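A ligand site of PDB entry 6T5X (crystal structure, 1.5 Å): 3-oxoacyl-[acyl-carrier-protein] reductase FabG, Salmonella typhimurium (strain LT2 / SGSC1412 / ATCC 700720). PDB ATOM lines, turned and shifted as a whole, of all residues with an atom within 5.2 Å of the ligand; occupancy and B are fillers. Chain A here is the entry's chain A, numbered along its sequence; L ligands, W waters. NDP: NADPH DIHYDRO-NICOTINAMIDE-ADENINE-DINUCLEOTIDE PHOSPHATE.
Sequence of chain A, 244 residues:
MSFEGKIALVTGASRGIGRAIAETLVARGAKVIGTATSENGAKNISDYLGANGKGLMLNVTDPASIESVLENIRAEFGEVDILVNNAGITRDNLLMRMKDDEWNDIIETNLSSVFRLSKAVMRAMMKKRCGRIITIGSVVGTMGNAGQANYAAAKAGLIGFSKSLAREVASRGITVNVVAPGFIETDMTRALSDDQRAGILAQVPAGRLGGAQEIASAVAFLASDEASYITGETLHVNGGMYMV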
ATOM      1  N   GLY A  12      12.752 -11.830   4.374  1.00  0.00           N
ATOM      2  CA  GLY A  12      12.725 -13.285   4.276  1.00  0.00           C
ATOM      3  C   GLY A  12      12.769 -13.806   2.853  1.00  0.00           C
ATOM      4  O   GLY A  12      11.895 -14.572   2.458  1.00  0.00           O
ATOM      5  N   ALA A  13      13.835 -13.468   2.129  1.00  0.00           N
ATOM      6  CA  ALA A  13      13.983 -13.763   0.707  1.00  0.00           C
ATOM      7  C   ALA A  13      14.968 -14.902   0.443  1.00  0.00           C
ATOM      8  O   ALA A  13      15.424 -15.062  -0.675  1.00  0.00           O
ATOM      9  CB  ALA A  13      14.419 -12.501  -0.030  1.00  0.00           C
ATOM     10  N   SER A  14      15.270 -15.706   1.475  1.00  0.00           N
ATOM     11  CA  SER A  14      16.178 -16.850   1.330  1.00  0.00           C
ATOM     12  C   SER A  14      15.742 -17.924   0.379  1.00  0.00           C
ATOM     13  O   SER A  14      16.570 -18.508  -0.324  1.00  0.00           O
ATOM     14  CB  SER A  14      16.323 -17.553   2.674  1.00  0.00           C
ATOM     15  OG  SER A  14      16.798 -16.664   3.615  1.00  0.00           O
ATOM     16  N   ARG A  15      14.451 -18.245   0.431  1.00  0.00           N
ATOM     17  CA  ARG A  15      13.886 -19.322  -0.336  1.00  0.00           C
ATOM     18  C   ARG A  15      12.377 -19.153  -0.449  1.00  0.00           C
ATOM     19  O   ARG A  15      11.834 -18.150   0.024  1.00  0.00           O
ATOM     20  CB  ARG A  15      14.198 -20.650   0.335  1.00  0.00           C
ATOM     21  CG  ARG A  15      13.402 -20.905   1.604  1.00  0.00           C
ATOM     22  CD  ARG A  15      14.050 -21.970   2.438  1.00  0.00           C
ATOM     23  NE  ARG A  15      15.260 -21.446   3.061  1.00  0.00           N
ATOM     24  CZ  ARG A  15      15.310 -20.763   4.210  1.00  0.00           C
ATOM     25  NH1 ARG A  15      14.218 -20.519   4.930  1.00  0.00           N
ATOM     26  NH2 ARG A  15      16.494 -20.329   4.649  1.00  0.00           N
ATOM     27  N   GLY A  16      11.734 -20.123  -1.098  1.00  0.00           N
ATOM     28  CA  GLY A  16      10.281 -20.220  -1.165  1.00  0.00           C
ATOM     29  C   GLY A  16       9.667 -18.976  -1.759  1.00  0.00           C
ATOM     30  O   GLY A  16      10.138 -18.470  -2.778  1.00  0.00           O
ATOM     31  N   ILE A  17       8.610 -18.514  -1.104  1.00  0.00           N
ATOM     32  CA  ILE A  17       7.828 -17.375  -1.617  1.00  0.00           C
ATOM     33  C   ILE A  17       8.655 -16.089  -1.671  1.00  0.00           C
ATOM     34  O   ILE A  17       8.638 -15.377  -2.671  1.00  0.00           O
ATOM     35  CB  ILE A  17       6.571 -17.178  -0.745  1.00  0.00           C
ATOM     36  CG1 ILE A  17       5.631 -18.363  -0.931  1.00  0.00           C
ATOM     37  CG2 ILE A  17       5.889 -15.821  -1.029  1.00  0.00           C
ATOM     38  CD1 ILE A  17       4.561 -18.549   0.122  1.00  0.00           C
ATOM     39  N   GLY A  18       9.419 -15.820  -0.611  1.00  0.00           N
ATOM     40  CA  GLY A  18      10.231 -14.629  -0.581  1.00  0.00           C
ATOM     41  C   GLY A  18      11.276 -14.536  -1.676  1.00  0.00           C
ATOM     42  O   GLY A  18      11.447 -13.485  -2.309  1.00  0.00           O
ATOM     43  N   THR A  35      16.229 -10.188   2.461  1.00  0.00           N
ATOM     44  CA  THR A  35      16.800 -10.418   3.786  1.00  0.00           C
ATOM     45  C   THR A  35      16.714 -11.847   4.291  1.00  0.00           C
ATOM     46  O   THR A  35      15.861 -12.640   3.882  1.00  0.00           O
ATOM     47  CB  THR A  35      16.229  -9.476   4.867  1.00  0.00           C
ATOM     48  OG1 THR A  35      14.947  -9.926   5.274  1.00  0.00           O
ATOM     49  CG2 THR A  35      16.152  -8.069   4.364  1.00  0.00           C
ATOM     50  N   ALA A  36      17.681 -12.181   5.146  1.00  0.00           N
ATOM     51  CA  ALA A  36      17.701 -13.441   5.879  1.00  0.00           C
ATOM     52  C   ALA A  36      18.072 -13.136   7.326  1.00  0.00           C
ATOM     53  O   ALA A  36      18.544 -12.029   7.637  1.00  0.00           O
ATOM     54  CB  ALA A  36      18.724 -14.394   5.264  1.00  0.00           C
ATOM     55  N   THR A  37      17.890 -14.143   8.189  1.00  0.00           N
ATOM     56  CA  THR A  37      18.158 -13.974   9.633  1.00  0.00           C
ATOM     57  C   THR A  37      19.645 -14.152   9.988  1.00  0.00           C
ATOM     58  O   THR A  37      20.033 -13.917  11.128  1.00  0.00           O
ATOM     59  CB  THR A  37      17.323 -14.930  10.504  1.00  0.00           C
ATOM     60  OG1 THR A  37      17.628 -16.294  10.189  1.00  0.00           O
ATOM     61  CG2 THR A  37      15.820 -14.637  10.295  1.00  0.00           C
ATOM     62  N   SER A  38      20.452 -14.580   9.025  1.00  0.00           N
ATOM     63  CA  SER A  38      21.898 -14.751   9.252  1.00  0.00           C
ATOM     64  C   SER A  38      22.727 -14.112   8.141  1.00  0.00           C
ATOM     65  O   SER A  38      22.252 -13.905   7.022  1.00  0.00           O
ATOM     66  CB  SER A  38      22.207 -16.245   9.324  1.00  0.00           C
ATOM     67  OG  SER A  38      22.119 -16.879   8.051  1.00  0.00           O
ATOM     68  N   LEU A  58      18.546  -9.407   8.530  1.00  0.00           N
ATOM     69  CA  LEU A  58      17.496  -8.661   9.214  1.00  0.00           C
ATOM     70  C   LEU A  58      16.732  -9.590  10.141  1.00  0.00           C
ATOM     71  O   LEU A  58      16.346 -10.692   9.738  1.00  0.00           O
ATOM     72  CB  LEU A  58      16.512  -8.053   8.200  1.00  0.00           C
ATOM     73  CG  LEU A  58      15.249  -7.394   8.769  1.00  0.00           C
ATOM     74  CD1 LEU A  58      15.603  -6.134   9.557  1.00  0.00           C
ATOM     75  CD2 LEU A  58      14.279  -7.073   7.659  1.00  0.00           C
ATOM     76  N   ASN A  59      16.508  -9.128  11.369  1.00  0.00           N
ATOM     77  CA  ASN A  59      15.550  -9.730  12.292  1.00  0.00           C
ATOM     78  C   ASN A  59      14.389  -8.752  12.430  1.00  0.00           C
ATOM     79  O   ASN A  59      14.551  -7.686  13.016  1.00  0.00           O
ATOM     80  CB  ASN A  59      16.194  -9.951  13.673  1.00  0.00           C
ATOM     81  CG  ASN A  59      15.263 -10.601  14.671  1.00  0.00           C
ATOM     82  OD1 ASN A  59      14.082 -10.888  14.401  1.00  0.00           O
ATOM     83  ND2 ASN A  59      15.802 -10.852  15.880  1.00  0.00           N
ATOM     84  N   VAL A  60      13.216  -9.132  11.903  1.00  0.00           N
ATOM     85  CA  VAL A  60      12.040  -8.234  11.928  1.00  0.00           C
ATOM     86  C   VAL A  60      11.437  -8.022  13.326  1.00  0.00           C
ATOM     87  O   VAL A  60      10.536  -7.191  13.468  1.00  0.00           O
ATOM     88  CB  VAL A  60      10.928  -8.644  10.942  1.00  0.00           C
ATOM     89  CG1 VAL A  60      11.448  -8.695   9.510  1.00  0.00           C
ATOM     90  CG2 VAL A  60      10.264  -9.947  11.320  1.00  0.00           C
ATOM     91  N   THR A  61      11.913  -8.751  14.344  1.00  0.00           N
ATOM     92  CA  THR A  61      11.506  -8.512  15.743  1.00  0.00           C
ATOM     93  C   THR A  61      12.436  -7.566  16.498  1.00  0.00           C
ATOM     94  O   THR A  61      12.112  -7.187  17.629  1.00  0.00           O
ATOM     95  CB  THR A  61      11.378  -9.824  16.548  1.00  0.00           C
ATOM     96  OG1 THR A  61      12.673 -10.409  16.781  1.00  0.00           O
ATOM     97  CG2 THR A  61      10.517 -10.812  15.821  1.00  0.00           C
ATOM     98  N   ASN A  86       7.255 -10.332   3.876  1.00  0.00           N
ATOM     99  CA  ASN A  86       7.120 -11.768   3.644  1.00  0.00           C
ATOM    100  C   ASN A  86       7.601 -12.613   4.829  1.00  0.00           C
ATOM    101  O   ASN A  86       7.105 -13.716   5.004  1.00  0.00           O
ATOM    102  CB  ASN A  86       7.848 -12.168   2.340  1.00  0.00           C
ATOM    103  CG  ASN A  86       7.933 -13.676   2.157  1.00  0.00           C
ATOM    104  OD1 ASN A  86       6.990 -14.320   1.731  1.00  0.00           O
ATOM    105  ND2 ASN A  86       9.081 -14.266   2.542  1.00  0.00           N
ATOM    106  N   ALA A  87       8.526 -12.103   5.642  1.00  0.00           N
ATOM    107  CA  ALA A  87       9.038 -12.901   6.768  1.00  0.00           C
ATOM    108  C   ALA A  87       7.917 -13.413   7.660  1.00  0.00           C
ATOM    109  O   ALA A  87       6.956 -12.696   7.964  1.00  0.00           O
ATOM    110  CB  ALA A  87      10.023 -12.101   7.589  1.00  0.00           C
ATOM    111  N   GLY A  88       8.020 -14.672   8.067  1.00  0.00           N
ATOM    112  CA  GLY A  88       7.004 -15.270   8.922  1.00  0.00           C
ATOM    113  C   GLY A  88       7.373 -16.693   9.302  1.00  0.00           C
ATOM    114  O   GLY A  88       8.149 -17.345   8.613  1.00  0.00           O
ATOM    115  N   ILE A  89       6.825 -17.142  10.424  1.00  0.00           N
ATOM    116  CA  ILE A  89       7.095 -18.453  10.989  1.00  0.00           C
ATOM    117  C   ILE A  89       5.793 -19.119  11.401  1.00  0.00           C
ATOM    118  O   ILE A  89       4.738 -18.468  11.470  1.00  0.00           O
ATOM    119  CB  ILE A  89       8.048 -18.365  12.217  1.00  0.00           C
ATOM    120  CG1 ILE A  89       7.457 -17.436  13.298  1.00  0.00           C
ATOM    121  CG2 ILE A  89       9.415 -17.873  11.785  1.00  0.00           C
ATOM    122  CD1 ILE A  89       8.229 -17.364  14.586  1.00  0.00           C
ATOM    123  N   THR A 109       6.777 -11.980  15.337  1.00  0.00           N
ATOM    124  CA  THR A 109       7.379 -12.226  14.045  1.00  0.00           C
ATOM    125  C   THR A 109       6.416 -11.964  12.889  1.00  0.00           C
ATOM    126  O   THR A 109       6.839 -11.434  11.872  1.00  0.00           O
ATOM    127  CB  THR A 109       7.945 -13.630  13.944  1.00  0.00           C
ATOM    128  OG1 THR A 109       8.832 -13.841  15.060  1.00  0.00           O
ATOM    129  CG2 THR A 109       8.721 -13.821  12.647  1.00  0.00           C
ATOM    130  N   ASN A 110       5.145 -12.326  13.078  1.00  0.00           N
ATOM    131  CA  ASN A 110       4.156 -12.312  11.997  1.00  0.00           C
ATOM    132  C   ASN A 110       3.224 -11.107  11.983  1.00  0.00           C
ATOM    133  O   ASN A 110       2.625 -10.828  10.947  1.00  0.00           O
ATOM    134  CB  ASN A 110       3.315 -13.579  12.002  1.00  0.00           C
ATOM    135  CG  ASN A 110       4.110 -14.834  11.676  1.00  0.00           C
ATOM    136  OD1 ASN A 110       5.335 -14.837  11.686  1.00  0.00           O
ATOM    137  ND2 ASN A 110       3.405 -15.913  11.384  1.00  0.00           N
ATOM    138  N   ILE A 136       2.427 -10.543   3.109  1.00  0.00           N
ATOM    139  CA  ILE A 136       2.025 -11.893   2.809  1.00  0.00           C
ATOM    140  C   ILE A 136       1.265 -12.423   4.004  1.00  0.00           C
ATOM    141  O   ILE A 136       1.811 -12.621   5.112  1.00  0.00           O
ATOM    142  CB  ILE A 136       3.240 -12.796   2.460  1.00  0.00           C
ATOM    143  CG1 ILE A 136       4.144 -12.118   1.419  1.00  0.00           C
ATOM    144  CG2 ILE A 136       2.741 -14.156   2.038  1.00  0.00           C
ATOM    145  CD1 ILE A 136       3.443 -11.766   0.125  1.00  0.00           C
ATOM    146  N   GLY A 137      -0.028 -12.606   3.782  1.00  0.00           N
ATOM    147  CA  GLY A 137      -0.940 -13.132   4.777  1.00  0.00           C
ATOM    148  C   GLY A 137      -1.027 -14.625   4.650  1.00  0.00           C
ATOM    149  O   GLY A 137      -0.032 -15.288   4.377  1.00  0.00           O
ATOM    150  N   SER A 138      -2.219 -15.158   4.859  1.00  0.00           N
ATOM    151  CA  SER A 138      -2.509 -16.576   4.647  1.00  0.00           C
ATOM    152  C   SER A 138      -3.981 -16.797   4.560  1.00  0.00           C
ATOM    153  O   SER A 138      -4.747 -16.144   5.276  1.00  0.00           O
ATOM    154  CB  SER A 138      -1.960 -17.431   5.807  1.00  0.00           C
ATOM    155  OG  SER A 138      -2.347 -18.783   5.667  1.00  0.00           O
ATOM    156  N   VAL A 139      -4.396 -17.813   3.789  1.00  0.00           N
ATOM    157  CA  VAL A 139      -5.755 -18.295   3.862  1.00  0.00           C
ATOM    158  C   VAL A 139      -6.200 -18.526   5.303  1.00  0.00           C
ATOM    159  O   VAL A 139      -7.337 -18.279   5.661  1.00  0.00           O
ATOM    160  CB  VAL A 139      -5.964 -19.582   2.983  1.00  0.00           C
ATOM    161  CG1 VAL A 139      -5.217 -20.778   3.564  1.00  0.00           C
ATOM    162  CG2 VAL A 139      -7.445 -19.884   2.841  1.00  0.00           C
ATOM    163  N   TYR A 151      -1.033 -18.259  14.639  1.00  0.00           N
ATOM    164  CA  TYR A 151      -0.755 -17.880  13.258  1.00  0.00           C
ATOM    165  C   TYR A 151      -1.963 -17.142  12.671  1.00  0.00           C
ATOM    166  O   TYR A 151      -1.814 -16.095  12.061  1.00  0.00           O
ATOM    167  CB  TYR A 151      -0.438 -19.128  12.475  1.00  0.00           C
ATOM    168  CG  TYR A 151       0.040 -18.973  11.054  1.00  0.00           C
ATOM    169  CD1 TYR A 151       1.367 -18.641  10.777  1.00  0.00           C
ATOM    170  CD2 TYR A 151      -0.837 -19.176   9.983  1.00  0.00           C
ATOM    171  CE1 TYR A 151       1.805 -18.516   9.478  1.00  0.00           C
ATOM    172  CE2 TYR A 151      -0.381 -19.088   8.678  1.00  0.00           C
ATOM    173  CZ  TYR A 151       0.916 -18.731   8.434  1.00  0.00           C
ATOM    174  OH  TYR A 151       1.318 -18.671   7.135  1.00  0.00           O
ATOM    175  N   LYS A 155      -2.169 -13.443  11.148  1.00  0.00           N
ATOM    176  CA  LYS A 155      -2.471 -13.264   9.709  1.00  0.00           C
ATOM    177  C   LYS A 155      -3.792 -12.531   9.489  1.00  0.00           C
ATOM    178  O   LYS A 155      -3.914 -11.765   8.535  1.00  0.00           O
ATOM    179  CB  LYS A 155      -2.447 -14.605   8.985  1.00  0.00           C
ATOM    180  CG  LYS A 155      -1.070 -15.283   8.970  1.00  0.00           C
ATOM    181  CD  LYS A 155       0.007 -14.460   8.306  1.00  0.00           C
ATOM    182  CE  LYS A 155       1.245 -15.279   7.909  1.00  0.00           C
ATOM    183  NZ  LYS A 155       2.236 -14.466   7.195  1.00  0.00           N
ATOM    184  N   PRO A 181      -1.829 -16.339   0.454  1.00  0.00           N
ATOM    185  CA  PRO A 181      -1.675 -17.643  -0.176  1.00  0.00           C
ATOM    186  C   PRO A 181      -2.447 -18.738   0.502  1.00  0.00           C
ATOM    187  O   PRO A 181      -2.658 -18.699   1.719  1.00  0.00           O
ATOM    188  CB  PRO A 181      -0.171 -17.925  -0.021  1.00  0.00           C
ATOM    189  CG  PRO A 181       0.475 -16.612   0.264  1.00  0.00           C
ATOM    190  CD  PRO A 181      -0.574 -15.931   1.108  1.00  0.00           C
ATOM    191  N   GLY A 182      -2.876 -19.725  -0.273  1.00  0.00           N
ATOM    192  CA  GLY A 182      -3.301 -21.020   0.257  1.00  0.00           C
ATOM    193  C   GLY A 182      -2.047 -21.844   0.526  1.00  0.00           C
ATOM    194  O   GLY A 182      -1.015 -21.296   0.829  1.00  0.00           O
ATOM    195  N   PHE A 183      -2.130 -23.153   0.340  1.00  0.00           N
ATOM    196  CA  PHE A 183      -0.954 -24.008   0.594  1.00  0.00           C
ATOM    197  C   PHE A 183      -0.033 -23.989  -0.619  1.00  0.00           C
ATOM    198  O   PHE A 183      -0.481 -24.243  -1.744  1.00  0.00           O
ATOM    199  CB  PHE A 183      -1.434 -25.388   1.025  1.00  0.00           C
ATOM    200  CG  PHE A 183      -1.869 -25.396   2.457  1.00  0.00           C
ATOM    201  CD1 PHE A 183      -3.008 -24.675   2.857  1.00  0.00           C
ATOM    202  CD2 PHE A 183      -1.110 -26.025   3.434  1.00  0.00           C
ATOM    203  CE1 PHE A 183      -3.408 -24.635   4.198  1.00  0.00           C
ATOM    204  CE2 PHE A 183      -1.505 -25.994   4.766  1.00  0.00           C
ATOM    205  CZ  PHE A 183      -2.646 -25.293   5.152  1.00  0.00           C
ATOM    206  N   ILE A 184       1.226 -23.620  -0.373  1.00  0.00           N
ATOM    207  CA  ILE A 184       2.229 -23.404  -1.410  1.00  0.00           C
ATOM    208  C   ILE A 184       3.375 -24.394  -1.149  1.00  0.00           C
ATOM    209  O   ILE A 184       3.787 -24.560  -0.001  1.00  0.00           O
ATOM    210  CB  ILE A 184       2.802 -21.983  -1.357  1.00  0.00           C
ATOM    211  CG1 ILE A 184       1.669 -20.947  -1.367  1.00  0.00           C
ATOM    212  CG2 ILE A 184       3.761 -21.769  -2.513  1.00  0.00           C
ATOM    213  CD1 ILE A 184       0.726 -21.035  -2.545  1.00  0.00           C
ATOM    214  N   THR A 186       6.636 -25.280  -0.315  1.00  0.00           N
ATOM    215  CA  THR A 186       7.847 -24.614   0.266  1.00  0.00           C
ATOM    216  C   THR A 186       8.402 -25.447   1.431  1.00  0.00           C
ATOM    217  O   THR A 186       7.903 -26.543   1.682  1.00  0.00           O
ATOM    218  CB  THR A 186       7.602 -23.146   0.760  1.00  0.00           C
ATOM    219  OG1 THR A 186       6.971 -23.116   2.052  1.00  0.00           O
ATOM    220  CG2 THR A 186       6.748 -22.349  -0.202  1.00  0.00           C
ATOM    221  N   ASP A 187       9.420 -24.922   2.133  1.00  0.00           N
ATOM    222  CA  ASP A 187       9.921 -25.543   3.380  1.00  0.00           C
ATOM    223  C   ASP A 187       8.935 -25.428   4.553  1.00  0.00           C
ATOM    224  O   ASP A 187       9.129 -26.105   5.570  1.00  0.00           O
ATOM    225  CB  ASP A 187      11.261 -24.926   3.816  1.00  0.00           C
ATOM    226  CG  ASP A 187      12.429 -25.337   2.929  1.00  0.00           C
ATOM    227  OD1 ASP A 187      12.285 -26.212   2.061  1.00  0.00           O
ATOM    228  OD2 ASP A 187      13.504 -24.760   3.133  1.00  0.00           O
ATOM    229  N   MET A 188       7.914 -24.576   4.446  1.00  0.00           N
ATOM    230  CA  MET A 188       6.859 -24.557   5.458  1.00  0.00           C
ATOM    231  C   MET A 188       5.919 -25.763   5.325  1.00  0.00           C
ATOM    232  O   MET A 188       5.405 -26.255   6.337  1.00  0.00           O
ATOM    233  CB  MET A 188       6.074 -23.240   5.410  1.00  0.00           C
ATOM    234  CG  MET A 188       5.872 -22.577   6.753  1.00  0.00           C
ATOM    235  SD  MET A 188       4.963 -21.040   6.526  1.00  0.00           S
ATOM    236  CE  MET A 188       5.955 -19.920   7.510  1.00  0.00           C
ATOM    237  N   THR A 189       5.707 -26.244   4.088  1.00  0.00           N
ATOM    238  CA  THR A 189       4.724 -27.310   3.794  1.00  0.00           C
ATOM    239  C   THR A 189       5.300 -28.732   3.651  1.00  0.00           C
ATOM    240  O   THR A 189       4.694 -29.677   4.142  1.00  0.00           O
ATOM    241  CB  THR A 189       3.932 -26.981   2.511  1.00  0.00           C
ATOM    242  OG1 THR A 189       4.839 -26.586   1.468  1.00  0.00           O
ATOM    243  CG2 THR A 189       2.940 -25.852   2.771  1.00  0.00           C
HETATM  244  PA  NDP L   1      10.003 -20.094   4.704  1.00  0.00           P
HETATM  245  O1A NDP L   1       9.947 -20.705   6.076  1.00  0.00           O
HETATM  246  O2A NDP L   1      10.572 -20.852   3.506  1.00  0.00           O
HETATM  247  O5B NDP L   1      10.763 -18.718   4.749  1.00  0.00           O
HETATM  248  C5B NDP L   1      10.577 -17.793   5.815  1.00  0.00           C
HETATM  249  C4B NDP L   1      11.489 -16.611   5.581  1.00  0.00           C
HETATM  250  O4B NDP L   1      11.295 -15.687   6.643  1.00  0.00           O
HETATM  251  C3B NDP L   1      12.972 -17.003   5.596  1.00  0.00           C
HETATM  252  O3B NDP L   1      13.700 -16.250   4.626  1.00  0.00           O
HETATM  253  C2B NDP L   1      13.398 -16.649   7.006  1.00  0.00           C
HETATM  254  O2B NDP L   1      14.784 -16.351   7.138  1.00  0.00           O
HETATM  255  C1B NDP L   1      12.539 -15.432   7.290  1.00  0.00           C
HETATM  256  N9A NDP L   1      12.387 -15.169   8.729  1.00  0.00           N
HETATM  257  C8A NDP L   1      11.920 -15.987   9.701  1.00  0.00           C
HETATM  258  N7A NDP L   1      11.938 -15.380  10.895  1.00  0.00           N
HETATM  259  C5A NDP L   1      12.437 -14.145  10.701  1.00  0.00           C
HETATM  260  C6A NDP L   1      12.730 -12.976  11.552  1.00  0.00           C
HETATM  261  N6A NDP L   1      12.513 -13.022  12.880  1.00  0.00           N
HETATM  262  N1A NDP L   1      13.228 -11.871  10.939  1.00  0.00           N
HETATM  263  C2A NDP L   1      13.455 -11.834   9.615  1.00  0.00           C
HETATM  264  N3A NDP L   1      13.216 -12.865   8.778  1.00  0.00           N
HETATM  265  C4A NDP L   1      12.712 -14.018   9.274  1.00  0.00           C
HETATM  266  O3  NDP L   1       8.431 -19.668   4.465  1.00  0.00           O
HETATM  267  PN  NDP L   1       7.470 -19.514   3.189  1.00  0.00           P
HETATM  268  O1N NDP L   1       8.250 -19.070   1.974  1.00  0.00           O
HETATM  269  O2N NDP L   1       6.546 -20.689   3.110  1.00  0.00           O
HETATM  270  O5D NDP L   1       6.540 -18.334   3.757  1.00  0.00           O
HETATM  271  C5D NDP L   1       6.831 -16.975   3.524  1.00  0.00           C
HETATM  272  C4D NDP L   1       5.562 -16.243   3.965  1.00  0.00           C
HETATM  273  O4D NDP L   1       4.422 -16.818   3.348  1.00  0.00           O
HETATM  274  C3D NDP L   1       5.303 -16.340   5.469  1.00  0.00           C
HETATM  275  O3D NDP L   1       4.849 -15.062   5.939  1.00  0.00           O
HETATM  276  C2D NDP L   1       4.214 -17.372   5.614  1.00  0.00           C
HETATM  277  O2D NDP L   1       3.413 -17.191   6.777  1.00  0.00           O
HETATM  278  C1D NDP L   1       3.429 -17.123   4.338  1.00  0.00           C
HETATM  279  N1N NDP L   1       2.627 -18.240   3.857  1.00  0.00           N
HETATM  280  C2N NDP L   1       3.223 -19.379   3.451  1.00  0.00           C
HETATM  281  C3N NDP L   1       2.467 -20.440   2.974  1.00  0.00           C
HETATM  282  C7N NDP L   1       3.020 -21.745   2.512  1.00  0.00           C
HETATM  283  O7N NDP L   1       2.217 -22.593   2.153  1.00  0.00           O
HETATM  284  N7N NDP L   1       4.323 -21.989   2.492  1.00  0.00           N
HETATM  285  C4N NDP L   1       0.972 -20.310   2.864  1.00  0.00           C
HETATM  286  C5N NDP L   1       0.446 -19.041   3.302  1.00  0.00           C
HETATM  287  C6N NDP L   1       1.296 -18.057   3.738  1.00  0.00           C
HETATM  288  P2B NDP L   1      15.904 -17.540   7.172  1.00  0.00           P
HETATM  289  O1X NDP L   1      17.085 -16.714   7.654  1.00  0.00           O
HETATM  290  O2X NDP L   1      15.403 -18.565   8.154  1.00  0.00           O
HETATM  291  O3X NDP L   1      16.062 -18.087   5.797  1.00  0.00           O
HETATM  292  O   HOH W   1      11.313 -14.858  14.906  1.00  0.00           O
HETATM  293  O   HOH W   2       9.791 -17.121   1.970  1.00  0.00           O
HETATM  294  O   HOH W   3      14.421 -18.373  10.600  1.00  0.00           O
HETATM  295  O   HOH W   4      12.407 -17.655   2.546  1.00  0.00           O
HETATM  296  O   HOH W   5       9.326 -19.784   8.452  1.00  0.00           O
HETATM  297  O   HOH W   6      13.607 -20.495   7.286  1.00  0.00           O
HETATM  298  O   HOH W   7      -0.246 -20.458   5.867  1.00  0.00           O
HETATM  299  O   HOH W   8      12.527 -16.889  13.302  1.00  0.00           O
HETATM  300  O   HOH W   9      11.778 -19.325   9.186  1.00  0.00           O
HETATM  301  O   HOH W  10      19.640 -17.418   7.132  1.00  0.00           O
HETATM  302  O   HOH W  11      10.363 -23.243   6.851  1.00  0.00           O
HETATM  303  O   HOH W  12      17.034 -20.454   9.025  1.00  0.00           O
HETATM  304  O   HOH W  13      15.412 -11.754   7.289  1.00  0.00           O
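An oxygen (O3X) of the ligand is in salt-bridge range of the guanidinium group (NH2) of Arg 15, 2.6 Å away. OH of Tyr 151 lies within hydrogen-bond range of O2D of the ligand (2.6 Å). The backbone NH (N) of Thr 37 lies within hydrogen-bond range of an oxygen (O1X) of the ligand, at 2.7 Å. OG1 of Thr 37 sits at hydrogen-bond distance from O1X of the ligand (2.6 Å). The side-chain hydroxyl (OG1) of Thr 186 lies within hydrogen-bond range of an oxygen (O2N) of the ligand (2.7 Å). An oxygen (O3X) of the ligand sits at hydrogen-bond distance from the side-chain hydroxyl (OG) of Ser 14 (2.7 Å). O3D of the ligand sits at hydrogen-bond distance from O of Asn 86, 2.8 Å away. O7N of the ligand sits at hydrogen-bond distance from N of Ile 184. N1A of the ligand is in hydrogen-bond range of N of Val 60 (2.9 Å). NZ of Lys 155 lies within hydrogen-bond range of O3D of the ligand, at 3.0 Å. A nitrogen (N6A) of the ligand lies within hydrogen-bond range of the side-chain amide oxygen (OD1) of Asn 59 (3.1 Å). The backbone carbonyl oxygen (O) of Gly 12 lies close to an oxygen (O3B) of the ligand. An oxygen (O1N) of the ligand lies within hydrogen-bond range of the backbone NH (N) of Ile 17, at 3.1 Å.
The side-chain carboxylate (OD2) of Asp 187 lies within salt-bridge range of the guanidinium group (NE) of Arg 15 (3.8 Å). N of Thr 186 is in hydrogen-bond range of OG1 of Thr 189, at 2.8 Å. ND2 of Asn 86 lies within hydrogen-bond range of O of Gly 12 (2.8 Å). O of Ile 184 is in hydrogen-bond range of OG1 of Thr 189, 2.7 Å away. The side-chain amide oxygen of Asn 59 lies within hydrogen-bond range of the side-chain hydroxyl of Thr 61. N of Gly 12 sits at hydrogen-bond distance from OG1 of Thr 35 (3.0 Å). O of Ile 89 lies within hydrogen-bond range of ND2 of Asn 110, at 2.9 Å. The backbone NH (N) of Ala 13 lies within hydrogen-bond range of the backbone carbonyl oxygen (O) of Thr 35 (2.8 Å).
The side-chain sulfur (SD) of Met 188 sits close to an oxygen (O2N) of the ligand, 3.8 Å away. Merely in contact with the ligand: Gly 182, Leu 58, Gly 137, Thr 189, Ile 136, Ala 87, Pro 181, Ile 89, Ser 138, Gly 88, Ala 36, Ala 13, Phe 183, Thr 109 and Gly 16. 28 residues have an atom within 4 Å of the ligand: Gly 12, Ala 13, Ser 14, Arg 15, Gly 16, Ile 17, Ala 36, Thr 37, Leu 58, Asn 59, Val 60, Asn 86, Ala 87, Gly 88, Ile 89, Thr 109, Ile 136, Gly 137, Ser 138, Tyr 151, Lys 155, Pro 181, Gly 182, Phe 183, Ile 184, Thr 186, Met 188 and Thr 189.
Water W5 lies within hydrogen-bond range of an oxygen (O1A) of the ligand (2.6 Å) and the backbone carbonyl oxygen of Gly 88 (2.7 Å). Water W11 bridges an oxygen (O1A) of the ligand and the backbone carbonyl oxygen (O) of Asp 187. Water W6 bridges the guanidinium group (NH1) of Arg 15 (2.4 Å) and an oxygen (O2X) of the ligand (2.8 Å). Water W4 lies within hydrogen-bond range of the backbone carbonyl oxygen (O) of Arg 15 (2.6 Å), an oxygen (O3B) of the ligand (2.8 Å) and the backbone carbonyl oxygen (O) of Gly 12 (3.1 Å). Water W13 lies within hydrogen-bond range of the side-chain hydroxyl of Thr 35 (2.8 Å), the backbone carbonyl oxygen of Leu 58 (2.8 Å), a nitrogen (N3A) of the ligand (2.9 Å) and the backbone NH of Ala 36 (3.2 Å). Water W1 lies within hydrogen-bond range of the side-chain hydroxyl (OG1) of Thr 109 (2.7 Å) and a nitrogen (N6A) of the ligand (3.0 Å).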
